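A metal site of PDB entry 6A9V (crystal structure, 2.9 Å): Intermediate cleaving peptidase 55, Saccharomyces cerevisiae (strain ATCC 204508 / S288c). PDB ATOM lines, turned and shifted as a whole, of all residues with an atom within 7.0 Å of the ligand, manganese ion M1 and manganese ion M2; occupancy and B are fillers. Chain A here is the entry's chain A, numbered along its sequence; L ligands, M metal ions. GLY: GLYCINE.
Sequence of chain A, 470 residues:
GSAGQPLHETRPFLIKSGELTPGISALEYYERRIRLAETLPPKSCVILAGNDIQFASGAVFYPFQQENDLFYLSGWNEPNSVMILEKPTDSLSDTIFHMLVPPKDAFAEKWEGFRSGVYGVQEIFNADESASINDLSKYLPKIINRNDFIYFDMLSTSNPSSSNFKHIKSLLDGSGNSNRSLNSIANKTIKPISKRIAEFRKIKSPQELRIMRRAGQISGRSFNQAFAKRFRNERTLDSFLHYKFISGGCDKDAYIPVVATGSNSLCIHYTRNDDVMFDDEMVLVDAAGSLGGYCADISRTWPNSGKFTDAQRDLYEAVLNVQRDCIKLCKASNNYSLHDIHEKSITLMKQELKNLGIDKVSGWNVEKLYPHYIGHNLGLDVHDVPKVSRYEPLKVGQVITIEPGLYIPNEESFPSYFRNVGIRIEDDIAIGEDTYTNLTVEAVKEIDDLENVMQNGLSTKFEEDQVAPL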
ATOM      1  N   TYR A 255      -4.078 -18.727 -23.044  1.00  0.00           N
ATOM      2  CA  TYR A 255      -3.102 -18.140 -22.142  1.00  0.00           C
ATOM      3  C   TYR A 255      -3.828 -17.173 -21.229  1.00  0.00           C
ATOM      4  O   TYR A 255      -4.997 -16.834 -21.448  1.00  0.00           O
ATOM      5  CB  TYR A 255      -1.983 -17.424 -22.921  1.00  0.00           C
ATOM      6  CG  TYR A 255      -2.500 -16.499 -23.999  1.00  0.00           C
ATOM      7  CD1 TYR A 255      -2.662 -16.947 -25.307  1.00  0.00           C
ATOM      8  CD2 TYR A 255      -2.844 -15.190 -23.712  1.00  0.00           C
ATOM      9  CE1 TYR A 255      -3.141 -16.111 -26.287  1.00  0.00           C
ATOM     10  CE2 TYR A 255      -3.323 -14.345 -24.686  1.00  0.00           C
ATOM     11  CZ  TYR A 255      -3.476 -14.804 -25.976  1.00  0.00           C
ATOM     12  OH  TYR A 255      -3.949 -13.963 -26.963  1.00  0.00           O
ATOM     13  N   ILE A 256      -3.128 -16.710 -20.198  1.00  0.00           N
ATOM     14  CA  ILE A 256      -3.676 -15.732 -19.261  1.00  0.00           C
ATOM     15  C   ILE A 256      -3.850 -14.407 -19.996  1.00  0.00           C
ATOM     16  O   ILE A 256      -2.874 -13.859 -20.533  1.00  0.00           O
ATOM     17  CB  ILE A 256      -2.787 -15.593 -18.022  1.00  0.00           C
ATOM     18  CG1 ILE A 256      -2.783 -16.898 -17.213  1.00  0.00           C
ATOM     19  CG2 ILE A 256      -3.249 -14.425 -17.157  1.00  0.00           C
ATOM     20  CD1 ILE A 256      -1.802 -16.917 -16.069  1.00  0.00           C
ATOM     21  N   VAL A 258      -4.691 -10.409 -21.199  1.00  0.00           N
ATOM     22  CA  VAL A 258      -4.308  -9.050 -20.829  1.00  0.00           C
ATOM     23  C   VAL A 258      -5.454  -8.122 -21.227  1.00  0.00           C
ATOM     24  O   VAL A 258      -5.852  -8.096 -22.401  1.00  0.00           O
ATOM     25  CB  VAL A 258      -3.005  -8.623 -21.523  1.00  0.00           C
ATOM     26  CG1 VAL A 258      -2.678  -7.172 -21.185  1.00  0.00           C
ATOM     27  CG2 VAL A 258      -1.860  -9.542 -21.137  1.00  0.00           C
ATOM     28  N   VAL A 285      -6.087  -5.476 -25.434  1.00  0.00           N
ATOM     29  CA  VAL A 285      -6.579  -6.788 -25.040  1.00  0.00           C
ATOM     30  C   VAL A 285      -5.802  -7.855 -25.804  1.00  0.00           C
ATOM     31  O   VAL A 285      -5.831  -7.895 -27.033  1.00  0.00           O
ATOM     32  CB  VAL A 285      -8.081  -6.949 -25.299  1.00  0.00           C
ATOM     33  CG1 VAL A 285      -8.514  -8.382 -25.006  1.00  0.00           C
ATOM     34  CG2 VAL A 285      -8.867  -5.981 -24.430  1.00  0.00           C
ATOM     35  N   ASP A 286      -5.113  -8.721 -25.055  1.00  0.00           N
ATOM     36  CA  ASP A 286      -4.439  -9.889 -25.614  1.00  0.00           C
ATOM     37  C   ASP A 286      -5.113 -11.123 -25.020  1.00  0.00           C
ATOM     38  O   ASP A 286      -4.938 -11.415 -23.823  1.00  0.00           O
ATOM     39  CB  ASP A 286      -2.944  -9.869 -25.294  1.00  0.00           C
ATOM     40  CG  ASP A 286      -2.136 -10.793 -26.189  1.00  0.00           C
ATOM     41  OD1 ASP A 286      -2.667 -11.846 -26.596  1.00  0.00           O
ATOM     42  OD2 ASP A 286      -0.967 -10.470 -26.485  1.00  0.00           O
ATOM     43  N   ALA A 287      -5.891 -11.828 -25.835  1.00  0.00           N
ATOM     44  CA  ALA A 287      -6.655 -12.976 -25.376  1.00  0.00           C
ATOM     45  C   ALA A 287      -7.102 -13.784 -26.584  1.00  0.00           C
ATOM     46  O   ALA A 287      -7.360 -13.221 -27.654  1.00  0.00           O
ATOM     47  CB  ALA A 287      -7.860 -12.562 -24.529  1.00  0.00           C
ATOM     48  N   ALA A 296      -4.763 -20.115 -30.338  1.00  0.00           N
ATOM     49  CA  ALA A 296      -4.771 -18.869 -31.082  1.00  0.00           C
ATOM     50  C   ALA A 296      -4.117 -17.780 -30.237  1.00  0.00           C
ATOM     51  O   ALA A 296      -3.826 -17.975 -29.060  1.00  0.00           O
ATOM     52  CB  ALA A 296      -6.186 -18.481 -31.489  1.00  0.00           C
ATOM     53  N   ASP A 297      -3.892 -16.618 -30.849  1.00  0.00           N
ATOM     54  CA  ASP A 297      -3.255 -15.520 -30.143  1.00  0.00           C
ATOM     55  C   ASP A 297      -3.631 -14.216 -30.836  1.00  0.00           C
ATOM     56  O   ASP A 297      -3.190 -13.966 -31.955  1.00  0.00           O
ATOM     57  CB  ASP A 297      -1.737 -15.714 -30.110  1.00  0.00           C
ATOM     58  CG  ASP A 297      -1.065 -14.847 -29.066  1.00  0.00           C
ATOM     59  OD1 ASP A 297      -1.756 -14.022 -28.437  1.00  0.00           O
ATOM     60  OD2 ASP A 297       0.166 -15.005 -28.872  1.00  0.00           O
ATOM     61  N   ILE A 298      -4.427 -13.382 -30.160  1.00  0.00           N
ATOM     62  CA  ILE A 298      -4.972 -12.164 -30.750  1.00  0.00           C
ATOM     63  C   ILE A 298      -4.735 -11.002 -29.795  1.00  0.00           C
ATOM     64  O   ILE A 298      -4.958 -11.125 -28.587  1.00  0.00           O
ATOM     65  CB  ILE A 298      -6.472 -12.312 -31.061  1.00  0.00           C
ATOM     66  CG1 ILE A 298      -6.691 -13.349 -32.159  1.00  0.00           C
ATOM     67  CG2 ILE A 298      -7.078 -10.968 -31.470  1.00  0.00           C
ATOM     68  CD1 ILE A 298      -8.150 -13.571 -32.518  1.00  0.00           C
ATOM     69  N   SER A 299      -4.287  -9.878 -30.344  1.00  0.00           N
ATOM     70  CA  SER A 299      -4.242  -8.607 -29.622  1.00  0.00           C
ATOM     71  C   SER A 299      -5.027  -7.564 -30.408  1.00  0.00           C
ATOM     72  O   SER A 299      -4.959  -7.522 -31.639  1.00  0.00           O
ATOM     73  CB  SER A 299      -2.812  -8.110 -29.399  1.00  0.00           C
ATOM     74  OG  SER A 299      -2.070  -9.035 -28.613  1.00  0.00           O
ATOM     75  N   ILE A 374       8.777  -9.361 -32.850  1.00  0.00           N
ATOM     76  CA  ILE A 374       7.663  -9.200 -33.792  1.00  0.00           C
ATOM     77  C   ILE A 374       6.611 -10.283 -33.582  1.00  0.00           C
ATOM     78  O   ILE A 374       5.419 -10.050 -33.809  1.00  0.00           O
ATOM     79  CB  ILE A 374       8.185  -9.181 -35.235  1.00  0.00           C
ATOM     80  CG1 ILE A 374       7.057  -8.870 -36.219  1.00  0.00           C
ATOM     81  CG2 ILE A 374       8.834 -10.515 -35.593  1.00  0.00           C
ATOM     82  CD1 ILE A 374       6.330  -7.575 -35.920  1.00  0.00           C
ATOM     83  N   GLY A 375       7.027 -11.470 -33.159  1.00  0.00           N
ATOM     84  CA  GLY A 375       6.093 -12.559 -33.015  1.00  0.00           C
ATOM     85  C   GLY A 375       6.790 -13.835 -32.607  1.00  0.00           C
ATOM     86  O   GLY A 375       7.932 -13.820 -32.127  1.00  0.00           O
ATOM     87  N   HIS A 376       6.095 -14.956 -32.812  1.00  0.00           N
ATOM     88  CA  HIS A 376       6.577 -16.245 -32.339  1.00  0.00           C
ATOM     89  C   HIS A 376       5.823 -17.341 -33.079  1.00  0.00           C
ATOM     90  O   HIS A 376       4.718 -17.142 -33.582  1.00  0.00           O
ATOM     91  CB  HIS A 376       6.382 -16.390 -30.832  1.00  0.00           C
ATOM     92  CG  HIS A 376       4.986 -16.066 -30.372  1.00  0.00           C
ATOM     93  ND1 HIS A 376       3.971 -16.990 -30.387  1.00  0.00           N
ATOM     94  CD2 HIS A 376       4.454 -14.922 -29.885  1.00  0.00           C
ATOM     95  CE1 HIS A 376       2.860 -16.433 -29.930  1.00  0.00           C
ATOM     96  NE2 HIS A 376       3.131 -15.174 -29.621  1.00  0.00           N
ATOM     97  N   LEU A 378       3.501 -20.529 -33.376  1.00  0.00           N
ATOM     98  CA  LEU A 378       2.259 -20.812 -32.671  1.00  0.00           C
ATOM     99  C   LEU A 378       1.809 -22.233 -32.978  1.00  0.00           C
ATOM    100  O   LEU A 378       1.939 -22.704 -34.112  1.00  0.00           O
ATOM    101  CB  LEU A 378       1.168 -19.816 -33.073  1.00  0.00           C
ATOM    102  CG  LEU A 378      -0.121 -19.828 -32.255  1.00  0.00           C
ATOM    103  CD1 LEU A 378       0.136 -19.339 -30.838  1.00  0.00           C
ATOM    104  CD2 LEU A 378      -1.182 -18.979 -32.934  1.00  0.00           C
ATOM    105  N   VAL A 382       1.633 -21.586 -26.754  1.00  0.00           N
ATOM    106  CA  VAL A 382       1.519 -20.198 -27.205  1.00  0.00           C
ATOM    107  C   VAL A 382       2.815 -19.768 -27.886  1.00  0.00           C
ATOM    108  O   VAL A 382       2.829 -19.378 -29.062  1.00  0.00           O
ATOM    109  CB  VAL A 382       1.177 -19.266 -26.037  1.00  0.00           C
ATOM    110  CG1 VAL A 382       0.865 -17.866 -26.546  1.00  0.00           C
ATOM    111  CG2 VAL A 382       0.002 -19.812 -25.245  1.00  0.00           C
ATOM    112  N   HIS A 383       3.927 -19.845 -27.154  1.00  0.00           N
ATOM    113  CA  HIS A 383       5.247 -19.682 -27.746  1.00  0.00           C
ATOM    114  C   HIS A 383       5.728 -21.062 -28.162  1.00  0.00           C
ATOM    115  O   HIS A 383       6.504 -21.737 -27.469  1.00  0.00           O
ATOM    116  CB  HIS A 383       6.203 -19.007 -26.762  1.00  0.00           C
ATOM    117  CG  HIS A 383       5.768 -17.638 -26.343  1.00  0.00           C
ATOM    118  ND1 HIS A 383       6.472 -16.867 -25.438  1.00  0.00           N
ATOM    119  CD2 HIS A 383       4.696 -16.894 -26.713  1.00  0.00           C
ATOM    120  CE1 HIS A 383       5.854 -15.716 -25.270  1.00  0.00           C
ATOM    121  NE2 HIS A 383       4.777 -15.701 -26.032  1.00  0.00           N
ATOM    122  N   THR A 401       2.995 -15.459 -35.312  1.00  0.00           N
ATOM    123  CA  THR A 401       2.221 -14.261 -35.054  1.00  0.00           C
ATOM    124  C   THR A 401       2.982 -13.035 -35.520  1.00  0.00           C
ATOM    125  O   THR A 401       4.211 -13.036 -35.623  1.00  0.00           O
ATOM    126  CB  THR A 401       1.913 -14.129 -33.557  1.00  0.00           C
ATOM    127  OG1 THR A 401       3.128 -13.889 -32.830  1.00  0.00           O
ATOM    128  CG2 THR A 401       1.276 -15.404 -33.022  1.00  0.00           C
ATOM    129  N   ILE A 402       2.239 -11.975 -35.834  1.00  0.00           N
ATOM    130  CA  ILE A 402       2.798 -10.683 -36.208  1.00  0.00           C
ATOM    131  C   ILE A 402       2.182  -9.660 -35.257  1.00  0.00           C
ATOM    132  O   ILE A 402       1.023  -9.271 -35.442  1.00  0.00           O
ATOM    133  CB  ILE A 402       2.513 -10.325 -37.672  1.00  0.00           C
ATOM    134  CG1 ILE A 402       3.059 -11.410 -38.613  1.00  0.00           C
ATOM    135  CG2 ILE A 402       3.115  -8.966 -38.015  1.00  0.00           C
ATOM    136  CD1 ILE A 402       4.570 -11.437 -38.698  1.00  0.00           C
ATOM    137  N   GLU A 403       2.941  -9.231 -34.258  1.00  0.00           N
ATOM    138  CA  GLU A 403       2.417  -8.381 -33.187  1.00  0.00           C
ATOM    139  C   GLU A 403       3.376  -7.251 -32.860  1.00  0.00           C
ATOM    140  O   GLU A 403       4.018  -7.239 -31.817  1.00  0.00           O
ATOM    141  CB  GLU A 403       2.114  -9.221 -31.940  1.00  0.00           C
ATOM    142  CG  GLU A 403       3.215 -10.200 -31.562  1.00  0.00           C
ATOM    143  CD  GLU A 403       2.871 -11.009 -30.330  1.00  0.00           C
ATOM    144  OE1 GLU A 403       3.194 -12.219 -30.306  1.00  0.00           O
ATOM    145  OE2 GLU A 403       2.259 -10.442 -29.406  1.00  0.00           O
ATOM    146  N   ARG A 424      -1.110  -2.521 -29.383  1.00  0.00           N
ATOM    147  CA  ARG A 424      -0.574  -3.712 -30.014  1.00  0.00           C
ATOM    148  C   ARG A 424      -1.659  -4.373 -30.857  1.00  0.00           C
ATOM    149  O   ARG A 424      -2.813  -4.459 -30.427  1.00  0.00           O
ATOM    150  CB  ARG A 424      -0.014  -4.718 -28.990  1.00  0.00           C
ATOM    151  CG  ARG A 424       0.585  -5.967 -29.635  1.00  0.00           C
ATOM    152  CD  ARG A 424       1.419  -6.800 -28.671  1.00  0.00           C
ATOM    153  NE  ARG A 424       0.598  -7.518 -27.695  1.00  0.00           N
ATOM    154  CZ  ARG A 424       0.565  -7.226 -26.396  1.00  0.00           C
ATOM    155  NH1 ARG A 424       1.301  -6.233 -25.914  1.00  0.00           N
ATOM    156  NH2 ARG A 424      -0.204  -7.927 -25.580  1.00  0.00           N
ATOM    157  N   GLU A 426      -2.181  -7.939 -33.021  1.00  0.00           N
ATOM    158  CA  GLU A 426      -1.616  -9.269 -33.235  1.00  0.00           C
ATOM    159  C   GLU A 426      -2.568 -10.123 -34.048  1.00  0.00           C
ATOM    160  O   GLU A 426      -3.772 -10.172 -33.766  1.00  0.00           O
ATOM    161  CB  GLU A 426      -1.320  -9.944 -31.894  1.00  0.00           C
ATOM    162  CG  GLU A 426      -0.783 -11.351 -32.018  1.00  0.00           C
ATOM    163  CD  GLU A 426      -0.370 -11.937 -30.685  1.00  0.00           C
ATOM    164  OE1 GLU A 426      -0.876 -11.472 -29.638  1.00  0.00           O
ATOM    165  OE2 GLU A 426       0.473 -12.861 -30.680  1.00  0.00           O
ATOM    166  N   ASP A 428      -2.518 -14.130 -36.372  1.00  0.00           N
ATOM    167  CA  ASP A 428      -1.849 -15.418 -36.547  1.00  0.00           C
ATOM    168  C   ASP A 428      -1.774 -15.736 -38.032  1.00  0.00           C
ATOM    169  O   ASP A 428      -2.810 -15.887 -38.690  1.00  0.00           O
ATOM    170  CB  ASP A 428      -2.572 -16.517 -35.784  1.00  0.00           C
ATOM    171  CG  ASP A 428      -2.687 -16.221 -34.307  1.00  0.00           C
ATOM    172  OD1 ASP A 428      -1.851 -15.454 -33.804  1.00  0.00           O
ATOM    173  OD2 ASP A 428      -3.609 -16.749 -33.652  1.00  0.00           O
HETATM  174  N   GLY L   1      -0.220 -13.854 -25.686  1.00  0.00           N
HETATM  175  CA  GLY L   1       1.139 -13.439 -25.388  1.00  0.00           C
HETATM  176  C   GLY L   1       1.955 -13.152 -26.622  1.00  0.00           C
HETATM  177  O   GLY L   1       1.745 -12.148 -27.304  1.00  0.00           O
HETATM  178  OXT GLY L   1       2.854 -13.908 -26.976  1.00  0.00           O
HETATM  179 MN    MN M   1       1.788 -13.605 -29.156  1.00  0.00          MN
HETATM  180 MN    MN M   2      -0.600 -12.241 -27.652  1.00  0.00          MN
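Manganese ion M1 is bound by a ring nitrogen (NE2) of His 376 (2.1 Å), the side-chain carboxylate (OE2) of Glu 426 (2.1 Å), the side-chain carboxylate (OD2) of Asp 297 (2.2 Å), the side-chain carboxylate (OE1) of Glu 403 (2.3 Å), an oxygen (O) of the ligand (2.4 Å) and an oxygen (OXT) of the ligand (2.4 Å).
Merely in contact with manganese ion M2: Tyr 255 (3.8 Å) and Ser 299 (3.7 Å).
Of the 22 residues printed, 6 come within 4 Å of manganese ion M2.
The nearest printed residue that does not touch manganese ion M2 is Ile 298 (4.6 Å).
An oxygen (OXT) of the ligand sits close to a ring nitrogen (NE2) of His 383 (2.8 Å).
Residues that only touch manganese ion M1: Thr 401 (3.9 Å).
The nearest printed residue that does not touch manganese ion M1 is His 383 (4.8 Å).
N of Thr 401 lies within hydrogen-bond range of O of His 376 (3.0 Å).
A ring nitrogen (ND1) of His 376 lies within hydrogen-bond range of the backbone carbonyl oxygen (O) of Val 382 (3.0 Å).
O of Ser 299 is in hydrogen-bond range of N of Glu 426 (3.1 Å).
The side-chain carboxylate (OD1) of Asp 286 sits close to the side-chain hydroxyl (OH) of Tyr 255 (2.5 Å).
OD2 of Asp 286 sits close to OG of Ser 299.
OE2 of Glu 403 is in salt-bridge range of NE of Arg 424 (3.8 Å).
OH of Tyr 255 is in hydrogen-bond range of N of Ile 298 (3.3 Å).
The side-chain hydroxyl of Tyr 255 sits at hydrogen-bond distance from the backbone NH of Ala 287, at 3.1 Å.
Manganese ion M2 is bound by the side-chain carboxylate (OE1) of Glu 426 (2.1 Å), the side-chain carboxylate (OD2) of Asp 286 (2.2 Å), the side-chain carboxylate (OD1) of Asp 297 (2.3 Å), the side-chain carboxylate (OD1) of Asp 286 (2.4 Å), an oxygen (O) of the ligand (2.4 Å) and a nitrogen (N) of the ligand (2.6 Å).
Manganese ion M2 has six donor atoms within binding distance.
CE2 of Tyr 255 touches N of the ligand, at 3.3 Å.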
